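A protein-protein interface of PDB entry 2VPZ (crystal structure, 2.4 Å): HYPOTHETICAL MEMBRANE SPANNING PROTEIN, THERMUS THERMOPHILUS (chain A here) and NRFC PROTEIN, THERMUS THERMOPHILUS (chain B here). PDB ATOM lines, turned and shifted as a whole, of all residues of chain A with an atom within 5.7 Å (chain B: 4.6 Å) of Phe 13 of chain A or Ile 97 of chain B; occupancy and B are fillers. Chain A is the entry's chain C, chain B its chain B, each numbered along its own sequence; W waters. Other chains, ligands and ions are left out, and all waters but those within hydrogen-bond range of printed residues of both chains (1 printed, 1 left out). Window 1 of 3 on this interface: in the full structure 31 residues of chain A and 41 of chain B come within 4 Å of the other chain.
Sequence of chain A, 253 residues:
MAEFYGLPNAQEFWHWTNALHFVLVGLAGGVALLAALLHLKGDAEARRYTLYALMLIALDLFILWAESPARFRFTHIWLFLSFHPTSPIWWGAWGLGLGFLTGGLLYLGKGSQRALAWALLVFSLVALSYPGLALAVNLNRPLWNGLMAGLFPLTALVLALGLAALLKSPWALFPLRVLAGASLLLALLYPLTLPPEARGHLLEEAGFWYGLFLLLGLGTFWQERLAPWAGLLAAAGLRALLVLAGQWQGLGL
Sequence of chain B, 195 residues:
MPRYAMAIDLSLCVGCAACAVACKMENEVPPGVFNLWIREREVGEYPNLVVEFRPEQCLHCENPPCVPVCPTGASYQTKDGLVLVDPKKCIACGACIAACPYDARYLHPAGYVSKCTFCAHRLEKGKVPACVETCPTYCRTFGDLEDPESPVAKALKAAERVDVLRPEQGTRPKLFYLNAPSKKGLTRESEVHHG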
ATOM      1  N   ASN A   9      -9.085  26.820   6.399  1.00  0.00           N
ATOM      2  CA  ASN A   9      -8.772  25.405   6.180  1.00  0.00           C
ATOM      3  C   ASN A   9      -7.972  25.252   4.867  1.00  0.00           C
ATOM      4  O   ASN A   9      -8.486  24.740   3.871  1.00  0.00           O
ATOM      5  CB  ASN A   9     -10.073  24.600   6.117  1.00  0.00           C
ATOM      6  CG  ASN A   9     -10.943  24.789   7.355  1.00  0.00           C
ATOM      7  OD1 ASN A   9     -12.032  25.363   7.287  1.00  0.00           O
ATOM      8  ND2 ASN A   9     -10.455  24.319   8.490  1.00  0.00           N
ATOM      9  N   GLN A  11      -4.880  23.612   4.507  1.00  0.00           N
ATOM     10  CA  GLN A  11      -3.897  22.533   4.627  1.00  0.00           C
ATOM     11  C   GLN A  11      -4.071  21.435   3.548  1.00  0.00           C
ATOM     12  O   GLN A  11      -5.143  21.276   2.964  1.00  0.00           O
ATOM     13  CB  GLN A  11      -3.940  21.888   6.026  1.00  0.00           C
ATOM     14  CG  GLN A  11      -5.274  21.188   6.383  1.00  0.00           C
ATOM     15  CD  GLN A  11      -6.379  22.156   6.864  1.00  0.00           C
ATOM     16  OE1 GLN A  11      -7.570  21.798   6.919  1.00  0.00           O
ATOM     17  NE2 GLN A  11      -5.976  23.378   7.240  1.00  0.00           N
ATOM     18  N   GLU A  12      -2.995  20.699   3.302  1.00  0.00           N
ATOM     19  CA  GLU A  12      -2.947  19.600   2.341  1.00  0.00           C
ATOM     20  C   GLU A  12      -4.111  18.598   2.558  1.00  0.00           C
ATOM     21  O   GLU A  12      -4.253  18.032   3.645  1.00  0.00           O
ATOM     22  CB  GLU A  12      -1.592  18.884   2.466  1.00  0.00           C
ATOM     23  CG  GLU A  12      -1.353  17.726   1.519  1.00  0.00           C
ATOM     24  CD  GLU A  12      -0.214  16.813   1.977  1.00  0.00           C
ATOM     25  OE1 GLU A  12      -0.421  16.047   2.948  1.00  0.00           O
ATOM     26  OE2 GLU A  12       0.880  16.899   1.383  1.00  0.00           O
ATOM     27  N   PHE A  13      -4.943  18.403   1.529  1.00  0.00           N
ATOM     28  CA  PHE A  13      -6.086  17.474   1.565  1.00  0.00           C
ATOM     29  C   PHE A  13      -5.771  16.108   0.898  1.00  0.00           C
ATOM     30  O   PHE A  13      -6.471  15.128   1.154  1.00  0.00           O
ATOM     31  CB  PHE A  13      -7.353  18.118   0.927  1.00  0.00           C
ATOM     32  CG  PHE A  13      -7.110  18.852  -0.403  1.00  0.00           C
ATOM     33  CD1 PHE A  13      -7.235  18.191  -1.640  1.00  0.00           C
ATOM     34  CD2 PHE A  13      -6.716  20.198  -0.412  1.00  0.00           C
ATOM     35  CE1 PHE A  13      -6.966  18.865  -2.870  1.00  0.00           C
ATOM     36  CE2 PHE A  13      -6.440  20.889  -1.629  1.00  0.00           C
ATOM     37  CZ  PHE A  13      -6.564  20.216  -2.859  1.00  0.00           C
ATOM     38  N   TRP A  14      -4.743  16.055   0.039  1.00  0.00           N
ATOM     39  CA  TRP A  14      -4.291  14.811  -0.650  1.00  0.00           C
ATOM     40  C   TRP A  14      -2.810  14.580  -0.278  1.00  0.00           C
ATOM     41  O   TRP A  14      -1.940  15.348  -0.702  1.00  0.00           O
ATOM     42  CB  TRP A  14      -4.472  14.877  -2.194  1.00  0.00           C
ATOM     43  CG  TRP A  14      -5.939  14.750  -2.669  1.00  0.00           C
ATOM     44  CD1 TRP A  14      -6.970  14.140  -1.991  1.00  0.00           C
ATOM     45  CD2 TRP A  14      -6.543  15.305  -3.874  1.00  0.00           C
ATOM     46  NE1 TRP A  14      -8.154  14.294  -2.682  1.00  0.00           N
ATOM     47  CE2 TRP A  14      -7.926  15.003  -3.831  1.00  0.00           C
ATOM     48  CE3 TRP A  14      -6.050  16.035  -4.975  1.00  0.00           C
ATOM     49  CZ2 TRP A  14      -8.829  15.402  -4.857  1.00  0.00           C
ATOM     50  CZ3 TRP A  14      -6.945  16.439  -6.005  1.00  0.00           C
ATOM     51  CH2 TRP A  14      -8.318  16.119  -5.925  1.00  0.00           C
ATOM     52  N   HIS A  15      -2.563  13.519   0.494  1.00  0.00           N
ATOM     53  CA  HIS A  15      -1.267  13.129   1.047  1.00  0.00           C
ATOM     54  C   HIS A  15      -0.339  12.259   0.177  1.00  0.00           C
ATOM     55  O   HIS A  15      -0.660  11.986  -0.982  1.00  0.00           O
ATOM     56  CB  HIS A  15      -1.602  12.507   2.434  1.00  0.00           C
ATOM     57  CG  HIS A  15      -2.552  13.285   3.283  1.00  0.00           C
ATOM     58  ND1 HIS A  15      -2.222  14.498   3.801  1.00  0.00           N
ATOM     59  CD2 HIS A  15      -3.835  13.075   3.615  1.00  0.00           C
ATOM     60  CE1 HIS A  15      -3.262  15.022   4.402  1.00  0.00           C
ATOM     61  NE2 HIS A  15      -4.263  14.172   4.306  1.00  0.00           N
ATOM     62  N   ASN A 140      -9.367  27.169  -9.609  1.00  0.00           N
ATOM     63  CA  ASN A 140      -8.969  28.037  -8.492  1.00  0.00           C
ATOM     64  C   ASN A 140      -7.506  27.769  -8.091  1.00  0.00           C
ATOM     65  O   ASN A 140      -6.824  28.616  -7.485  1.00  0.00           O
ATOM     66  CB  ASN A 140      -9.885  27.827  -7.277  1.00  0.00           C
ATOM     67  CG  ASN A 140     -10.084  26.348  -6.933  1.00  0.00           C
ATOM     68  OD1 ASN A 140      -9.857  25.905  -5.794  1.00  0.00           O
ATOM     69  ND2 ASN A 140     -10.509  25.573  -7.925  1.00  0.00           N
ATOM     70  N   ARG A 141      -7.030  26.564  -8.414  1.00  0.00           N
ATOM     71  CA  ARG A 141      -5.648  26.118  -8.148  1.00  0.00           C
ATOM     72  C   ARG A 141      -4.787  26.494  -9.383  1.00  0.00           C
ATOM     73  O   ARG A 141      -4.815  25.784 -10.379  1.00  0.00           O
ATOM     74  CB  ARG A 141      -5.622  24.580  -7.935  1.00  0.00           C
ATOM     75  CG  ARG A 141      -6.667  23.998  -6.950  1.00  0.00           C
ATOM     76  CD  ARG A 141      -6.242  24.163  -5.472  1.00  0.00           C
ATOM     77  NE  ARG A 141      -7.327  23.935  -4.499  1.00  0.00           N
ATOM     78  CZ  ARG A 141      -7.246  24.139  -3.183  1.00  0.00           C
ATOM     79  NH1 ARG A 141      -6.118  24.583  -2.633  1.00  0.00           N
ATOM     80  NH2 ARG A 141      -8.293  23.900  -2.395  1.00  0.00           N
ATOM     81  N   TRP A 144      -2.669  23.578 -11.450  1.00  0.00           N
ATOM     82  CA  TRP A 144      -3.410  22.530 -12.163  1.00  0.00           C
ATOM     83  C   TRP A 144      -4.114  23.024 -13.399  1.00  0.00           C
ATOM     84  O   TRP A 144      -5.340  22.908 -13.526  1.00  0.00           O
ATOM     85  CB  TRP A 144      -4.410  21.864 -11.212  1.00  0.00           C
ATOM     86  CG  TRP A 144      -3.694  21.064 -10.185  1.00  0.00           C
ATOM     87  CD1 TRP A 144      -2.379  20.647 -10.235  1.00  0.00           C
ATOM     88  CD2 TRP A 144      -4.214  20.552  -8.953  1.00  0.00           C
ATOM     89  NE1 TRP A 144      -2.070  19.914  -9.119  1.00  0.00           N
ATOM     90  CE2 TRP A 144      -3.177  19.834  -8.318  1.00  0.00           C
ATOM     91  CE3 TRP A 144      -5.476  20.615  -8.328  1.00  0.00           C
ATOM     92  CZ2 TRP A 144      -3.355  19.191  -7.056  1.00  0.00           C
ATOM     93  CZ3 TRP A 144      -5.664  19.980  -7.083  1.00  0.00           C
ATOM     94  CH2 TRP A 144      -4.609  19.274  -6.468  1.00  0.00           C
ATOM     95  N   GLN A 247      -1.629  21.913  -4.671  1.00  0.00           N
ATOM     96  CA  GLN A 247      -2.722  22.168  -3.689  1.00  0.00           C
ATOM     97  C   GLN A 247      -2.519  23.540  -3.056  1.00  0.00           C
ATOM     98  O   GLN A 247      -2.284  23.665  -1.860  1.00  0.00           O
ATOM     99  CB  GLN A 247      -2.720  21.103  -2.571  1.00  0.00           C
ATOM    100  CG  GLN A 247      -3.106  19.708  -3.056  1.00  0.00           C
ATOM    101  CD  GLN A 247      -2.828  18.566  -2.056  1.00  0.00           C
ATOM    102  OE1 GLN A 247      -3.413  18.495  -0.967  1.00  0.00           O
ATOM    103  NE2 GLN A 247      -1.932  17.653  -2.442  1.00  0.00           N
ATOM    104  N   GLN A 249      -4.041  27.804  -3.510  1.00  0.00           N
ATOM    105  CA  GLN A 249      -5.078  28.748  -4.033  1.00  0.00           C
ATOM    106  C   GLN A 249      -4.413  30.048  -4.481  1.00  0.00           C
ATOM    107  O   GLN A 249      -4.878  30.777  -5.389  1.00  0.00           O
ATOM    108  CB  GLN A 249      -6.008  29.155  -2.929  1.00  0.00           C
ATOM    109  CG  GLN A 249      -6.589  28.101  -2.065  1.00  0.00           C
ATOM    110  CD  GLN A 249      -7.966  27.779  -2.539  1.00  0.00           C
ATOM    111  OE1 GLN A 249      -8.845  27.368  -1.783  1.00  0.00           O
ATOM    112  NE2 GLN A 249      -8.180  28.002  -3.837  1.00  0.00           N
ATOM    113  N   GLY B  94     -12.377  14.284  -0.900  1.00  0.00           N
ATOM    114  CA  GLY B  94     -11.747  15.603  -0.927  1.00  0.00           C
ATOM    115  C   GLY B  94     -11.820  16.420  -2.213  1.00  0.00           C
ATOM    116  O   GLY B  94     -11.116  17.424  -2.381  1.00  0.00           O
ATOM    117  N   ALA B  95     -12.680  15.988  -3.127  1.00  0.00           N
ATOM    118  CA  ALA B  95     -12.872  16.638  -4.418  1.00  0.00           C
ATOM    119  C   ALA B  95     -13.423  18.060  -4.246  1.00  0.00           C
ATOM    120  O   ALA B  95     -13.003  18.992  -4.946  1.00  0.00           O
ATOM    121  CB  ALA B  95     -13.836  15.795  -5.318  1.00  0.00           C
ATOM    122  N   CYS B  96     -14.355  18.198  -3.304  1.00  0.00           N
ATOM    123  CA  CYS B  96     -15.036  19.458  -2.931  1.00  0.00           C
ATOM    124  C   CYS B  96     -14.051  20.462  -2.276  1.00  0.00           C
ATOM    125  O   CYS B  96     -14.170  21.686  -2.448  1.00  0.00           O
ATOM    126  CB  CYS B  96     -16.237  19.165  -2.017  1.00  0.00           C
ATOM    127  SG  CYS B  96     -15.866  18.094  -0.609  1.00  0.00           S
ATOM    128  N   ILE B  97     -13.066  19.945  -1.542  1.00  0.00           N
ATOM    129  CA  ILE B  97     -12.021  20.787  -0.949  1.00  0.00           C
ATOM    130  C   ILE B  97     -11.138  21.322  -2.115  1.00  0.00           C
ATOM    131  O   ILE B  97     -10.873  22.526  -2.173  1.00  0.00           O
ATOM    132  CB  ILE B  97     -11.120  20.020   0.079  1.00  0.00           C
ATOM    133  CG1 ILE B  97     -11.944  19.487   1.245  1.00  0.00           C
ATOM    134  CG2 ILE B  97     -10.023  20.972   0.582  1.00  0.00           C
ATOM    135  CD1 ILE B  97     -11.289  18.330   2.003  1.00  0.00           C
ATOM    136  N   ALA B  98     -10.703  20.457  -3.043  1.00  0.00           N
ATOM    137  CA  ALA B  98      -9.911  20.877  -4.222  1.00  0.00           C
ATOM    138  C   ALA B  98     -10.613  21.995  -5.045  1.00  0.00           C
ATOM    139  O   ALA B  98      -9.978  22.960  -5.526  1.00  0.00           O
ATOM    140  CB  ALA B  98      -9.634  19.656  -5.159  1.00  0.00           C
ATOM    141  N   ALA B  99     -11.926  21.848  -5.204  1.00  0.00           N
ATOM    142  CA  ALA B  99     -12.776  22.792  -5.947  1.00  0.00           C
ATOM    143  C   ALA B  99     -13.237  24.107  -5.232  1.00  0.00           C
ATOM    144  O   ALA B  99     -13.494  25.099  -5.912  1.00  0.00           O
ATOM    145  CB  ALA B  99     -14.024  22.036  -6.532  1.00  0.00           C
ATOM    146  N   CYS B 100     -13.352  24.145  -3.907  1.00  0.00           N
ATOM    147  CA  CYS B 100     -13.778  25.406  -3.213  1.00  0.00           C
ATOM    148  C   CYS B 100     -12.636  26.478  -3.253  1.00  0.00           C
ATOM    149  O   CYS B 100     -11.538  26.222  -2.745  1.00  0.00           O
ATOM    150  CB  CYS B 100     -14.193  25.138  -1.739  1.00  0.00           C
ATOM    151  SG  CYS B 100     -14.950  26.634  -0.740  1.00  0.00           S
ATOM    152  N   ARG B 105     -14.049  24.434   3.531  1.00  0.00           N
ATOM    153  CA  ARG B 105     -14.356  23.074   3.992  1.00  0.00           C
ATOM    154  C   ARG B 105     -13.206  22.215   4.590  1.00  0.00           C
ATOM    155  O   ARG B 105     -12.027  22.403   4.286  1.00  0.00           O
ATOM    156  CB  ARG B 105     -15.044  22.253   2.879  1.00  0.00           C
ATOM    157  CG  ARG B 105     -15.651  22.983   1.673  1.00  0.00           C
ATOM    158  CD  ARG B 105     -16.100  21.947   0.594  1.00  0.00           C
ATOM    159  NE  ARG B 105     -17.502  22.077   0.203  1.00  0.00           N
ATOM    160  CZ  ARG B 105     -18.438  21.134   0.232  1.00  0.00           C
ATOM    161  NH1 ARG B 105     -18.170  19.906   0.642  1.00  0.00           N
ATOM    162  NH2 ARG B 105     -19.673  21.444  -0.142  1.00  0.00           N
ATOM    163  N   VAL B 113     -16.897  15.020   5.189  1.00  0.00           N
ATOM    164  CA  VAL B 113     -16.508  16.419   5.070  1.00  0.00           C
ATOM    165  C   VAL B 113     -17.555  17.396   5.633  1.00  0.00           C
ATOM    166  O   VAL B 113     -18.749  17.162   5.512  1.00  0.00           O
ATOM    167  CB  VAL B 113     -16.079  16.746   3.582  1.00  0.00           C
ATOM    168  CG1 VAL B 113     -16.138  18.245   3.313  1.00  0.00           C
ATOM    169  CG2 VAL B 113     -14.632  16.208   3.338  1.00  0.00           C
HETATM  170  O   HOH W   1     -13.095  25.494  -8.488  1.00  0.00           O
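Of the printed residues of chain B, Asn 9 of chain A touches Arg 105.
Glu 12 of chain A touches none of the printed residues of chain B.
Of chain B, only Ile 97 and Ala 98 come within 4 Å of Phe 13 of chain A.
Of the printed residues of chain B, Arg 141 of chain A touches Ile 97 and Ala 98.
Gln 247 of chain A touches none of the printed residues of chain B.
Of the printed residues of chain A, Ile 97 of chain B touches Phe 13 and Arg 141.
Of the printed residues of chain A, Ala 99 of chain B touches Asn 140 (3.6 Å).
Of the printed residues of chain A, Cys 100 of chain B touches Asn 140 and Gln 249.
Printed residues of chain A within 4 Å of Arg 105 of chain B: Asn 9.
The nearest residue of chain A that does not touch Ile 97 of chain B is Asn 140 of chain A (5.1 Å).
The nearest printed residue of chain B that does not touch Arg 141 of chain A is Cys 100 of chain B (4.01 Å).
CB of Asn 9 of chain A touches O of Arg 105 of chain B (3.5 Å).
Phe 13 of chain A touches Ile 97 of chain B.
Ala 98 of chain B touches Phe 13 of chain A.
O of Gly 94 of chain B touches CZ2 of Trp 14 of chain A (3.9 Å).
Ala 98 of chain B touches Trp 14 of chain A (CB to CH2, 3.9 Å).
ND2 of Asn 140 of chain A touches O of Ala 99 of chain B, at 3.6 Å.
Of the 9 printed residues of chain B, 6 touch a printed residue of chain A.
Printed residues of chain B that touch a printed residue of chain A: Gly 94, Ile 97, Ala 98, Ala 99, Cys 100 and Arg 105.
Hydrophobic or aromatic side chains of chain A that line the printed part of chain B: Phe 13 and Trp 14.
Among the printed residues, no Asp or Glu carboxylate lies within 4 Å of a Lys or Arg side-chain nitrogen of the other chain.
The side-chain sulfur (SG) of Cys 96 of chain B sits close to the guanidinium group (NH1) of Arg 105 of chain B.
The side-chain amide oxygen (OE1) of Gln 247 of chain A sits at hydrogen-bond distance from the backbone NH (N) of Phe 13 of chain A, at 2.9 Å.
The backbone carbonyl oxygen (O) of Trp 14 of chain A is in hydrogen-bond range of the side-chain amide nitrogen (NE2) of Gln 247 of chain A (2.9 Å).
The side-chain amide oxygen (OD1) of Asn 140 of chain A lies within hydrogen-bond range of the guanidinium group (NE) of Arg 141 of chain A (3.5 Å).
The side-chain amide oxygen of Asn 140 of chain A is in hydrogen-bond range of the side-chain amide nitrogen of Gln 249 of chain A (3.3 Å).
The backbone carbonyl oxygen of Ile 97 of chain B lies within hydrogen-bond range of the guanidinium group of Arg 141 of chain A, 2.9 Å away.
The side-chain amide oxygen of Asn 140 of chain A lies close to the backbone carbonyl oxygen of Ala 98 of chain B (3.0 Å).
The backbone carbonyl oxygen (O) of Ala 98 of chain B is in hydrogen-bond range of the guanidinium group (NE) of Arg 141 of chain A, at 3.0 Å.
The backbone carbonyl oxygen (O) of Cys 100 of chain B lies close to the side-chain amide oxygen (OD1) of Asn 140 of chain A.
O of Cys 100 of chain B lies close to OE1 of Gln 249 of chain A (3.1 Å).
Water W1 lies within hydrogen-bond range of O of Ala 99 of chain B and ND2 of Asn 140 of chain A.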
